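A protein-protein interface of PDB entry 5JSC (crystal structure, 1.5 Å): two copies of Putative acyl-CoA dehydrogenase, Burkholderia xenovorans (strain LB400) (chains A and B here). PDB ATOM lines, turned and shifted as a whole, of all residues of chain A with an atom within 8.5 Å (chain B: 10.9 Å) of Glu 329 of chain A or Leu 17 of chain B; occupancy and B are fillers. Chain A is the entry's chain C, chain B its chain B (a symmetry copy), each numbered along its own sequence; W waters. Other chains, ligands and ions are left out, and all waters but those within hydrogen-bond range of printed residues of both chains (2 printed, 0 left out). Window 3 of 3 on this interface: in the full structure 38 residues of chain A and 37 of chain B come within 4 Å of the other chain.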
ATOM      1  N   THR A  88     -24.562   2.394  -3.442  1.00  0.00           N
ATOM      2  CA  THR A  88     -24.326   1.242  -4.310  1.00  0.00           C
ATOM      3  C   THR A  88     -22.928   0.686  -4.114  1.00  0.00           C
ATOM      4  O   THR A  88     -22.730  -0.532  -4.119  1.00  0.00           O
ATOM      5  CB  THR A  88     -24.516   1.628  -5.784  1.00  0.00           C
ATOM      6  OG1 THR A  88     -25.611   2.542  -5.911  1.00  0.00           O
ATOM      7  CG2 THR A  88     -24.806   0.392  -6.617  1.00  0.00           C
ATOM      8  N   ASP A 259     -32.379  -2.505 -11.410  1.00  0.00           N
ATOM      9  CA  ASP A 259     -31.279  -1.631 -11.811  1.00  0.00           C
ATOM     10  C   ASP A 259     -30.350  -1.334 -10.647  1.00  0.00           C
ATOM     11  O   ASP A 259     -29.143  -1.143 -10.850  1.00  0.00           O
ATOM     12  CB  ASP A 259     -31.818  -0.324 -12.382  1.00  0.00           C
ATOM     13  CG  ASP A 259     -32.279  -0.457 -13.812  1.00  0.00           C
ATOM     14  OD1 ASP A 259     -31.922  -1.459 -14.470  1.00  0.00           O
ATOM     15  OD2 ASP A 259     -32.993   0.459 -14.284  1.00  0.00           O
ATOM     16  N   ARG A 320     -17.320   1.198 -11.511  1.00  0.00           N
ATOM     17  CA  ARG A 320     -17.766   2.286 -12.378  1.00  0.00           C
ATOM     18  C   ARG A 320     -19.277   2.431 -12.302  1.00  0.00           C
ATOM     19  O   ARG A 320     -19.797   3.534 -12.118  1.00  0.00           O
ATOM     20  CB  ARG A 320     -17.318   2.046 -13.828  1.00  0.00           C
ATOM     21  CG  ARG A 320     -17.687   3.169 -14.815  1.00  0.00           C
ATOM     22  CD  ARG A 320     -19.118   3.055 -15.374  1.00  0.00           C
ATOM     23  NE  ARG A 320     -19.301   1.844 -16.177  1.00  0.00           N
ATOM     24  CZ  ARG A 320     -19.118   1.791 -17.494  1.00  0.00           C
ATOM     25  NH1 ARG A 320     -18.763   2.874 -18.170  1.00  0.00           N
ATOM     26  NH2 ARG A 320     -19.291   0.645 -18.141  1.00  0.00           N
ATOM     27  N   ALA A 321     -20.001   1.317 -12.442  1.00  0.00           N
ATOM     28  CA  ALA A 321     -21.459   1.376 -12.376  1.00  0.00           C
ATOM     29  C   ALA A 321     -21.938   1.830 -11.004  1.00  0.00           C
ATOM     30  O   ALA A 321     -22.865   2.648 -10.903  1.00  0.00           O
ATOM     31  CB  ALA A 321     -22.066   0.015 -12.727  1.00  0.00           C
ATOM     32  N   ALA A 322     -21.330   1.312  -9.935  1.00  0.00           N
ATOM     33  CA  ALA A 322     -21.776   1.694  -8.595  1.00  0.00           C
ATOM     34  C   ALA A 322     -21.474   3.161  -8.317  1.00  0.00           C
ATOM     35  O   ALA A 322     -22.330   3.891  -7.796  1.00  0.00           O
ATOM     36  CB  ALA A 322     -21.125   0.793  -7.542  1.00  0.00           C
ATOM     37  N   TRP A 323     -20.275   3.618  -8.688  1.00  0.00           N
ATOM     38  CA  TRP A 323     -19.942   5.032  -8.536  1.00  0.00           C
ATOM     39  C   TRP A 323     -20.917   5.910  -9.318  1.00  0.00           C
ATOM     40  O   TRP A 323     -21.393   6.939  -8.813  1.00  0.00           O
ATOM     41  CB  TRP A 323     -18.496   5.274  -8.988  1.00  0.00           C
ATOM     42  CG  TRP A 323     -18.169   6.725  -9.157  1.00  0.00           C
ATOM     43  CD1 TRP A 323     -17.721   7.591  -8.189  1.00  0.00           C
ATOM     44  CD2 TRP A 323     -18.294   7.491 -10.355  1.00  0.00           C
ATOM     45  NE1 TRP A 323     -17.557   8.847  -8.721  1.00  0.00           N
ATOM     46  CE2 TRP A 323     -17.903   8.816 -10.048  1.00  0.00           C
ATOM     47  CE3 TRP A 323     -18.697   7.191 -11.665  1.00  0.00           C
ATOM     48  CZ2 TRP A 323     -17.901   9.835 -11.002  1.00  0.00           C
ATOM     49  CZ3 TRP A 323     -18.692   8.213 -12.613  1.00  0.00           C
ATOM     50  CH2 TRP A 323     -18.292   9.515 -12.272  1.00  0.00           C
ATOM     51  N   LEU A 324     -21.238   5.514 -10.551  1.00  0.00           N
ATOM     52  CA  LEU A 324     -22.117   6.323 -11.387  1.00  0.00           C
ATOM     53  C   LEU A 324     -23.521   6.408 -10.797  1.00  0.00           C
ATOM     54  O   LEU A 324     -24.117   7.497 -10.748  1.00  0.00           O
ATOM     55  CB  LEU A 324     -22.147   5.749 -12.804  1.00  0.00           C
ATOM     56  CG  LEU A 324     -23.000   6.508 -13.818  1.00  0.00           C
ATOM     57  CD1 LEU A 324     -22.617   7.991 -13.871  1.00  0.00           C
ATOM     58  CD2 LEU A 324     -22.869   5.850 -15.199  1.00  0.00           C
ATOM     59  N   ARG A 325     -24.066   5.281 -10.336  1.00  0.00           N
ATOM     60  CA  ARG A 325     -25.380   5.329  -9.703  1.00  0.00           C
ATOM     61  C   ARG A 325     -25.346   6.212  -8.463  1.00  0.00           C
ATOM     62  O   ARG A 325     -26.319   6.931  -8.175  1.00  0.00           O
ATOM     63  CB  ARG A 325     -25.855   3.921  -9.338  1.00  0.00           C
ATOM     64  CG  ARG A 325     -27.321   3.905  -8.965  1.00  0.00           C
ATOM     65  CD  ARG A 325     -27.822   2.608  -8.327  1.00  0.00           C
ATOM     66  NE  ARG A 325     -29.132   2.897  -7.767  1.00  0.00           N
ATOM     67  CZ  ARG A 325     -29.377   3.206  -6.497  1.00  0.00           C
ATOM     68  NH1 ARG A 325     -28.416   3.185  -5.591  1.00  0.00           N
ATOM     69  NH2 ARG A 325     -30.612   3.487  -6.124  1.00  0.00           N
ATOM     70  N   ASP A 326     -24.222   6.211  -7.749  1.00  0.00           N
ATOM     71  CA  ASP A 326     -24.063   7.034  -6.554  1.00  0.00           C
ATOM     72  C   ASP A 326     -23.847   8.511  -6.867  1.00  0.00           C
ATOM     73  O   ASP A 326     -23.754   9.320  -5.928  1.00  0.00           O
ATOM     74  CB  ASP A 326     -22.908   6.492  -5.706  1.00  0.00           C
ATOM     75  CG  ASP A 326     -23.248   5.162  -5.051  1.00  0.00           C
ATOM     76  OD1 ASP A 326     -24.449   4.811  -4.984  1.00  0.00           O
ATOM     77  OD2 ASP A 326     -22.326   4.468  -4.578  1.00  0.00           O
ATOM     78  N   GLN A 327     -23.758   8.886  -8.143  1.00  0.00           N
ATOM     79  CA  GLN A 327     -23.844  10.283  -8.544  1.00  0.00           C
ATOM     80  C   GLN A 327     -25.283  10.706  -8.794  1.00  0.00           C
ATOM     81  O   GLN A 327     -25.534  11.875  -9.127  1.00  0.00           O
ATOM     82  CB  GLN A 327     -23.010  10.544  -9.807  1.00  0.00           C
ATOM     83  CG  GLN A 327     -21.579  10.024  -9.735  1.00  0.00           C
ATOM     84  CD  GLN A 327     -20.846  10.526  -8.510  1.00  0.00           C
ATOM     85  OE1 GLN A 327     -20.616  11.731  -8.353  1.00  0.00           O
ATOM     86  NE2 GLN A 327     -20.477   9.604  -7.627  1.00  0.00           N
ATOM     87  N   GLY A 328     -26.227   9.783  -8.632  1.00  0.00           N
ATOM     88  CA  GLY A 328     -27.617  10.049  -8.928  1.00  0.00           C
ATOM     89  C   GLY A 328     -28.014   9.770 -10.356  1.00  0.00           C
ATOM     90  O   GLY A 328     -29.068  10.240 -10.794  1.00  0.00           O
ATOM     91  N   GLU A 329     -27.206   9.030 -11.103  1.00  0.00           N
ATOM     92  CA  GLU A 329     -27.467   8.787 -12.512  1.00  0.00           C
ATOM     93  C   GLU A 329     -28.082   7.412 -12.720  1.00  0.00           C
ATOM     94  O   GLU A 329     -27.856   6.481 -11.943  1.00  0.00           O
ATOM     95  CB  GLU A 329     -26.179   8.907 -13.328  1.00  0.00           C
ATOM     96  CG  GLU A 329     -25.596  10.301 -13.285  1.00  0.00           C
ATOM     97  CD  GLU A 329     -26.451  11.290 -14.045  1.00  0.00           C
ATOM     98  OE1 GLU A 329     -26.759  11.021 -15.224  1.00  0.00           O
ATOM     99  OE2 GLU A 329     -26.828  12.326 -13.460  1.00  0.00           O
ATOM    100  N   ASN A 330     -28.854   7.299 -13.797  1.00  0.00           N
ATOM    101  CA  ASN A 330     -29.359   6.009 -14.241  1.00  0.00           C
ATOM    102  C   ASN A 330     -28.204   5.131 -14.694  1.00  0.00           C
ATOM    103  O   ASN A 330     -27.268   5.607 -15.337  1.00  0.00           O
ATOM    104  CB  ASN A 330     -30.334   6.220 -15.398  1.00  0.00           C
ATOM    105  CG  ASN A 330     -30.741   4.931 -16.064  1.00  0.00           C
ATOM    106  OD1 ASN A 330     -30.057   4.428 -16.971  1.00  0.00           O
ATOM    107  ND2 ASN A 330     -31.874   4.387 -15.634  1.00  0.00           N
ATOM    108  N   VAL A 331     -28.268   3.837 -14.368  1.00  0.00           N
ATOM    109  CA  VAL A 331     -27.194   2.938 -14.779  1.00  0.00           C
ATOM    110  C   VAL A 331     -27.732   1.692 -15.477  1.00  0.00           C
ATOM    111  O   VAL A 331     -27.116   0.625 -15.396  1.00  0.00           O
ATOM    112  CB  VAL A 331     -26.302   2.535 -13.586  1.00  0.00           C
ATOM    113  CG1 VAL A 331     -25.489   3.721 -13.098  1.00  0.00           C
ATOM    114  CG2 VAL A 331     -27.130   1.923 -12.450  1.00  0.00           C
ATOM    115  N   THR A 332     -28.859   1.805 -16.194  1.00  0.00           N
ATOM    116  CA  THR A 332     -29.395   0.623 -16.873  1.00  0.00           C
ATOM    117  C   THR A 332     -28.334  -0.042 -17.752  1.00  0.00           C
ATOM    118  O   THR A 332     -28.147  -1.269 -17.702  1.00  0.00           O
ATOM    119  CB  THR A 332     -30.634   0.993 -17.697  1.00  0.00           C
ATOM    120  OG1 THR A 332     -31.608   1.616 -16.846  1.00  0.00           O
ATOM    121  CG2 THR A 332     -31.258  -0.263 -18.313  1.00  0.00           C
ATOM    122  N   GLU A 334     -24.853   0.514 -17.698  1.00  0.00           N
ATOM    123  CA  GLU A 334     -23.605   0.194 -17.016  1.00  0.00           C
ATOM    124  C   GLU A 334     -23.778  -0.956 -16.036  1.00  0.00           C
ATOM    125  O   GLU A 334     -22.854  -1.769 -15.872  1.00  0.00           O
ATOM    126  CB  GLU A 334     -23.082   1.444 -16.306  1.00  0.00           C
ATOM    127  CG  GLU A 334     -22.694   2.578 -17.259  1.00  0.00           C
ATOM    128  CD  GLU A 334     -23.865   3.453 -17.720  1.00  0.00           C
ATOM    129  OE1 GLU A 334     -25.028   3.197 -17.326  1.00  0.00           O
ATOM    130  OE2 GLU A 334     -23.614   4.419 -18.474  1.00  0.00           O
ATOM    131  N   GLU B  14     -21.582  21.547 -19.734  1.00  0.00           N
ATOM    132  CA  GLU B  14     -22.101  20.579 -18.777  1.00  0.00           C
ATOM    133  C   GLU B  14     -21.489  19.205 -19.014  1.00  0.00           C
ATOM    134  O   GLU B  14     -21.545  18.669 -20.122  1.00  0.00           O
ATOM    135  CB  GLU B  14     -23.626  20.497 -18.864  1.00  0.00           C
ATOM    136  N   LEU B  15     -20.910  18.636 -17.960  1.00  0.00           N
ATOM    137  CA  LEU B  15     -20.252  17.341 -18.068  1.00  0.00           C
ATOM    138  C   LEU B  15     -21.290  16.229 -18.169  1.00  0.00           C
ATOM    139  O   LEU B  15     -22.129  16.069 -17.275  1.00  0.00           O
ATOM    140  CB  LEU B  15     -19.338  17.121 -16.865  1.00  0.00           C
ATOM    141  CG  LEU B  15     -18.702  15.742 -16.677  1.00  0.00           C
ATOM    142  CD1 LEU B  15     -17.798  15.361 -17.851  1.00  0.00           C
ATOM    143  CD2 LEU B  15     -17.936  15.691 -15.364  1.00  0.00           C
ATOM    144  N   ASP B  16     -21.241  15.470 -19.261  1.00  0.00           N
ATOM    145  CA  ASP B  16     -22.057  14.268 -19.408  1.00  0.00           C
ATOM    146  C   ASP B  16     -21.554  13.214 -18.430  1.00  0.00           C
ATOM    147  O   ASP B  16     -20.460  12.669 -18.607  1.00  0.00           O
ATOM    148  CB  ASP B  16     -21.994  13.777 -20.850  1.00  0.00           C
ATOM    149  CG  ASP B  16     -22.716  12.457 -21.068  1.00  0.00           C
ATOM    150  OD1 ASP B  16     -23.415  11.973 -20.154  1.00  0.00           O
ATOM    151  OD2 ASP B  16     -22.590  11.901 -22.182  1.00  0.00           O
ATOM    152  N   LEU B  17     -22.342  12.927 -17.390  1.00  0.00           N
ATOM    153  CA  LEU B  17     -21.867  12.016 -16.357  1.00  0.00           C
ATOM    154  C   LEU B  17     -21.782  10.576 -16.834  1.00  0.00           C
ATOM    155  O   LEU B  17     -21.148   9.761 -16.160  1.00  0.00           O
ATOM    156  CB  LEU B  17     -22.752  12.095 -15.111  1.00  0.00           C
ATOM    157  CG  LEU B  17     -22.619  13.391 -14.312  1.00  0.00           C
ATOM    158  CD1 LEU B  17     -23.428  13.326 -13.024  1.00  0.00           C
ATOM    159  CD2 LEU B  17     -21.155  13.694 -14.021  1.00  0.00           C
ATOM    160  N   HIS B  18     -22.390  10.243 -17.967  1.00  0.00           N
ATOM    161  CA  HIS B  18     -22.226   8.911 -18.531  1.00  0.00           C
ATOM    162  C   HIS B  18     -20.992   8.787 -19.410  1.00  0.00           C
ATOM    163  O   HIS B  18     -20.675   7.676 -19.856  1.00  0.00           O
ATOM    164  CB  HIS B  18     -23.477   8.527 -19.319  1.00  0.00           C
ATOM    165  CG  HIS B  18     -24.681   8.336 -18.456  1.00  0.00           C
ATOM    166  ND1 HIS B  18     -25.085   7.096 -18.010  1.00  0.00           N
ATOM    167  CD2 HIS B  18     -25.554   9.231 -17.932  1.00  0.00           C
ATOM    168  CE1 HIS B  18     -26.168   7.234 -17.265  1.00  0.00           C
ATOM    169  NE2 HIS B  18     -26.471   8.518 -17.198  1.00  0.00           N
ATOM    170  N   SER B  19     -20.277   9.883 -19.653  1.00  0.00           N
ATOM    171  CA  SER B  19     -19.071   9.811 -20.462  1.00  0.00           C
ATOM    172  C   SER B  19     -17.895   9.342 -19.616  1.00  0.00           C
ATOM    173  O   SER B  19     -17.839   9.572 -18.402  1.00  0.00           O
ATOM    174  CB  SER B  19     -18.748  11.165 -21.090  1.00  0.00           C
ATOM    175  OG  SER B  19     -18.358  12.106 -20.109  1.00  0.00           O
ATOM    176  N   ALA B  20     -16.952   8.670 -20.273  1.00  0.00           N
ATOM    177  CA  ALA B  20     -15.786   8.169 -19.561  1.00  0.00           C
ATOM    178  C   ALA B  20     -14.960   9.304 -18.973  1.00  0.00           C
ATOM    179  O   ALA B  20     -14.308   9.126 -17.939  1.00  0.00           O
ATOM    180  CB  ALA B  20     -14.930   7.320 -20.496  1.00  0.00           C
ATOM    181  N   LEU B  21     -14.989  10.482 -19.597  1.00  0.00           N
ATOM    182  CA  LEU B  21     -14.217  11.595 -19.058  1.00  0.00           C
ATOM    183  C   LEU B  21     -14.732  12.059 -17.699  1.00  0.00           C
ATOM    184  O   LEU B  21     -14.006  12.771 -16.995  1.00  0.00           O
ATOM    185  CB  LEU B  21     -14.217  12.759 -20.046  1.00  0.00           C
ATOM    186  CG  LEU B  21     -13.264  12.569 -21.227  1.00  0.00           C
ATOM    187  CD1 LEU B  21     -13.531  13.613 -22.310  1.00  0.00           C
ATOM    188  CD2 LEU B  21     -11.815  12.650 -20.748  1.00  0.00           C
ATOM    189  N   ALA B  22     -15.949  11.669 -17.305  1.00  0.00           N
ATOM    190  CA  ALA B  22     -16.436  12.014 -15.975  1.00  0.00           C
ATOM    191  C   ALA B  22     -15.857  11.124 -14.883  1.00  0.00           C
ATOM    192  O   ALA B  22     -15.988  11.463 -13.699  1.00  0.00           O
ATOM    193  CB  ALA B  22     -17.967  11.961 -15.932  1.00  0.00           C
ATOM    194  N   TRP B  23     -15.219  10.013 -15.245  1.00  0.00           N
ATOM    195  CA  TRP B  23     -14.659   9.120 -14.240  1.00  0.00           C
ATOM    196  C   TRP B  23     -13.678   9.867 -13.343  1.00  0.00           C
ATOM    197  O   TRP B  23     -12.933  10.733 -13.822  1.00  0.00           O
ATOM    198  CB  TRP B  23     -13.919   7.953 -14.887  1.00  0.00           C
ATOM    199  CG  TRP B  23     -14.762   7.046 -15.708  1.00  0.00           C
ATOM    200  CD1 TRP B  23     -16.117   6.896 -15.658  1.00  0.00           C
ATOM    201  CD2 TRP B  23     -14.290   6.150 -16.711  1.00  0.00           C
ATOM    202  NE1 TRP B  23     -16.520   5.949 -16.577  1.00  0.00           N
ATOM    203  CE2 TRP B  23     -15.412   5.480 -17.238  1.00  0.00           C
ATOM    204  CE3 TRP B  23     -13.023   5.856 -17.225  1.00  0.00           C
ATOM    205  CZ2 TRP B  23     -15.304   4.537 -18.253  1.00  0.00           C
ATOM    206  CZ3 TRP B  23     -12.915   4.914 -18.230  1.00  0.00           C
ATOM    207  CH2 TRP B  23     -14.049   4.267 -18.736  1.00  0.00           C
ATOM    208  N   PRO B  24     -13.629   9.538 -12.048  1.00  0.00           N
ATOM    209  CA  PRO B  24     -12.701  10.225 -11.136  1.00  0.00           C
ATOM    210  C   PRO B  24     -11.243   9.850 -11.330  1.00  0.00           C
ATOM    211  O   PRO B  24     -10.393  10.367 -10.594  1.00  0.00           O
ATOM    212  CB  PRO B  24     -13.208   9.812  -9.740  1.00  0.00           C
ATOM    213  CG  PRO B  24     -13.991   8.555  -9.959  1.00  0.00           C
ATOM    214  CD  PRO B  24     -14.572   8.653 -11.341  1.00  0.00           C
ATOM    215  N   PHE B  26      -9.910  10.987 -13.828  1.00  0.00           N
ATOM    216  CA  PHE B  26      -9.532  12.190 -14.557  1.00  0.00           C
ATOM    217  C   PHE B  26      -9.647  13.422 -13.676  1.00  0.00           C
ATOM    218  O   PHE B  26     -10.503  13.492 -12.790  1.00  0.00           O
ATOM    219  CB  PHE B  26     -10.409  12.383 -15.796  1.00  0.00           C
ATOM    220  CG  PHE B  26     -10.223  11.308 -16.831  1.00  0.00           C
ATOM    221  CD1 PHE B  26      -9.024  11.204 -17.519  1.00  0.00           C
ATOM    222  CD2 PHE B  26     -11.238  10.405 -17.103  1.00  0.00           C
ATOM    223  CE1 PHE B  26      -8.832  10.217 -18.475  1.00  0.00           C
ATOM    224  CE2 PHE B  26     -11.061   9.414 -18.060  1.00  0.00           C
ATOM    225  CZ  PHE B  26      -9.856   9.324 -18.752  1.00  0.00           C
ATOM    226  N   ARG B  31     -10.144  16.800 -18.946  1.00  0.00           N
ATOM    227  CA  ARG B  31     -11.345  17.068 -19.729  1.00  0.00           C
ATOM    228  C   ARG B  31     -11.119  18.223 -20.698  1.00  0.00           C
ATOM    229  O   ARG B  31     -11.564  18.169 -21.849  1.00  0.00           O
ATOM    230  CB  ARG B  31     -12.518  17.339 -18.785  1.00  0.00           C
ATOM    231  CG  ARG B  31     -12.667  16.216 -17.760  1.00  0.00           C
ATOM    232  CD  ARG B  31     -13.820  16.385 -16.781  1.00  0.00           C
ATOM    233  NE  ARG B  31     -13.917  15.185 -15.949  1.00  0.00           N
ATOM    234  CZ  ARG B  31     -13.558  15.115 -14.670  1.00  0.00           C
ATOM    235  NH1 ARG B  31     -13.108  16.195 -14.041  1.00  0.00           N
ATOM    236  NH2 ARG B  31     -13.670  13.965 -14.013  1.00  0.00           N
ATOM    237  N   ASP B 312     -15.363  -0.429 -23.050  1.00  0.00           N
ATOM    238  CA  ASP B 312     -15.409   0.125 -21.689  1.00  0.00           C
ATOM    239  C   ASP B 312     -14.401  -0.564 -20.778  1.00  0.00           C
ATOM    240  O   ASP B 312     -13.731   0.097 -19.973  1.00  0.00           O
ATOM    241  CB  ASP B 312     -16.817   0.022 -21.085  1.00  0.00           C
ATOM    242  CG  ASP B 312     -17.726   1.172 -21.495  1.00  0.00           C
ATOM    243  OD1 ASP B 312     -17.350   1.947 -22.401  1.00  0.00           O
ATOM    244  OD2 ASP B 312     -18.835   1.289 -20.919  1.00  0.00           O
ATOM    245  N   LEU B 316     -11.354   1.460 -19.006  1.00  0.00           N
ATOM    246  CA  LEU B 316     -11.150   1.429 -17.559  1.00  0.00           C
ATOM    247  C   LEU B 316      -9.756   0.923 -17.206  1.00  0.00           C
ATOM    248  O   LEU B 316      -9.100   1.477 -16.315  1.00  0.00           O
ATOM    249  CB  LEU B 316     -12.238   0.579 -16.891  1.00  0.00           C
ATOM    250  CG  LEU B 316     -13.605   1.276 -16.847  1.00  0.00           C
ATOM    251  CD1 LEU B 316     -14.712   0.248 -16.693  1.00  0.00           C
ATOM    252  CD2 LEU B 316     -13.668   2.301 -15.707  1.00  0.00           C
HETATM  253  O   HOH W   1     -19.350   5.653 -17.501  1.00  0.00           O
HETATM  254  O   HOH W   2     -21.250   5.046 -19.501  1.00  0.00           O
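The side-chain carboxylate (OE2) of Glu 334 of chain A lies within hydrogen-bond range of a ring nitrogen (ND1) of His 18 of chain B. A ring nitrogen (NE2) of His 18 of chain B lies within hydrogen-bond range of the side-chain carboxylate (OE1) of Glu 329 of chain A, 3.2 Å away. The guanidinium group (NH2) of Arg 320 of chain A is in salt-bridge range of the side-chain carboxylate (OD2) of Asp 312 of chain B (2.9 Å).
O of Trp 323 of chain A is in hydrogen-bond range of NE2 of Gln 327 of chain A (3.1 Å). N of Glu 329 of chain A sits at hydrogen-bond distance from O of Leu 324 of chain A. NH2 of Arg 31 of chain B is in hydrogen-bond range of O of Ala 22 of chain B (3.4 Å). The backbone NH (N) of Thr 332 of chain A sits at hydrogen-bond distance from the side-chain amide oxygen (OD1) of Asn 330 of chain A (3.0 Å). The side-chain carboxylate of Asp 16 of chain B lies within hydrogen-bond range of the backbone NH of His 18 of chain B. The guanidinium group of Arg 31 of chain B sits at hydrogen-bond distance from the backbone carbonyl oxygen of Trp 23 of chain B, at 3.3 Å.
Among the printed residues, merely in contact across the chains: Arg 320 of chain A with Trp 23 of chain B (3.5 Å), Trp 323 of chain A with Ala 22 of chain B (3.3 Å), Trp 323 of chain A with Pro 24 of chain B (3.5 Å), Leu 324 of chain A with Leu 17 of chain B (3.2 Å), Leu 324 of chain A with His 18 of chain B (3.8 Å), Glu 329 of chain A with Leu 17 of chain B (3.6 Å) and Asn 330 of chain A with His 18 of chain B (2.8 Å).
Of chain B, only Leu 17 (3.6 Å) and His 18 (3.2 Å) come within 4 Å of Glu 329 of chain A. Of chain A, only Leu 324 (3.2 Å) and Glu 329 (3.6 Å) come within 4 Å of Leu 17 of chain B. Leu 324 of chain A touches just these residues of chain B: Leu 17 (3.2 Å) and His 18 (3.8 Å). No residue of chain B comes within 4 Å of Gly 328 of chain A. Of the printed residues of chain B, Asn 330 of chain A touches His 18. Of the printed residues of chain A, Asp 312 of chain B touches Arg 320. Printed residues of chain B within 4 Å of Glu 334 of chain A: His 18 (3.1 Å). Of the printed residues of chain A, Pro 24 of chain B touches Trp 323 (3.5 Å). Ala 322 of chain A touches none of the printed residues of chain B. Ala 20 of chain B touches none of the printed residues of chain A. The nearest residue of chain B that does not touch Glu 329 of chain A is Asp 16 of chain B (6.0 Å). The nearest printed residue of chain B that does not touch Arg 320 of chain A is Leu 316 of chain B (4.1 Å).
Hydrophobic or aromatic side chains of chain B that line the printed part of chain A: Leu 17, His 18, Trp 23 and Pro 24. Hydrophobic or aromatic side chains of chain A that line the printed part of chain B: Trp 323 and Leu 324. Among the printed residues, 10 pairs touch across the chains. Among the printed residues, Asp or Glu carboxylates within 4 Å of a Lys or Arg side-chain nitrogen of the other chain: Arg 320 of chain A with Asp 312 of chain B.
No position is printed for both chains.
Water W2 bridges the side-chain carboxylate of Glu 334 of chain A (2.7 Å) and the backbone carbonyl oxygen of His 18 of chain B (2.7 Å). Water W1 lies within hydrogen-bond range of the guanidinium group of Arg 320 of chain A, the indole nitrogen of Trp 23 of chain B and the backbone carbonyl oxygen of His 18 of chain B.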
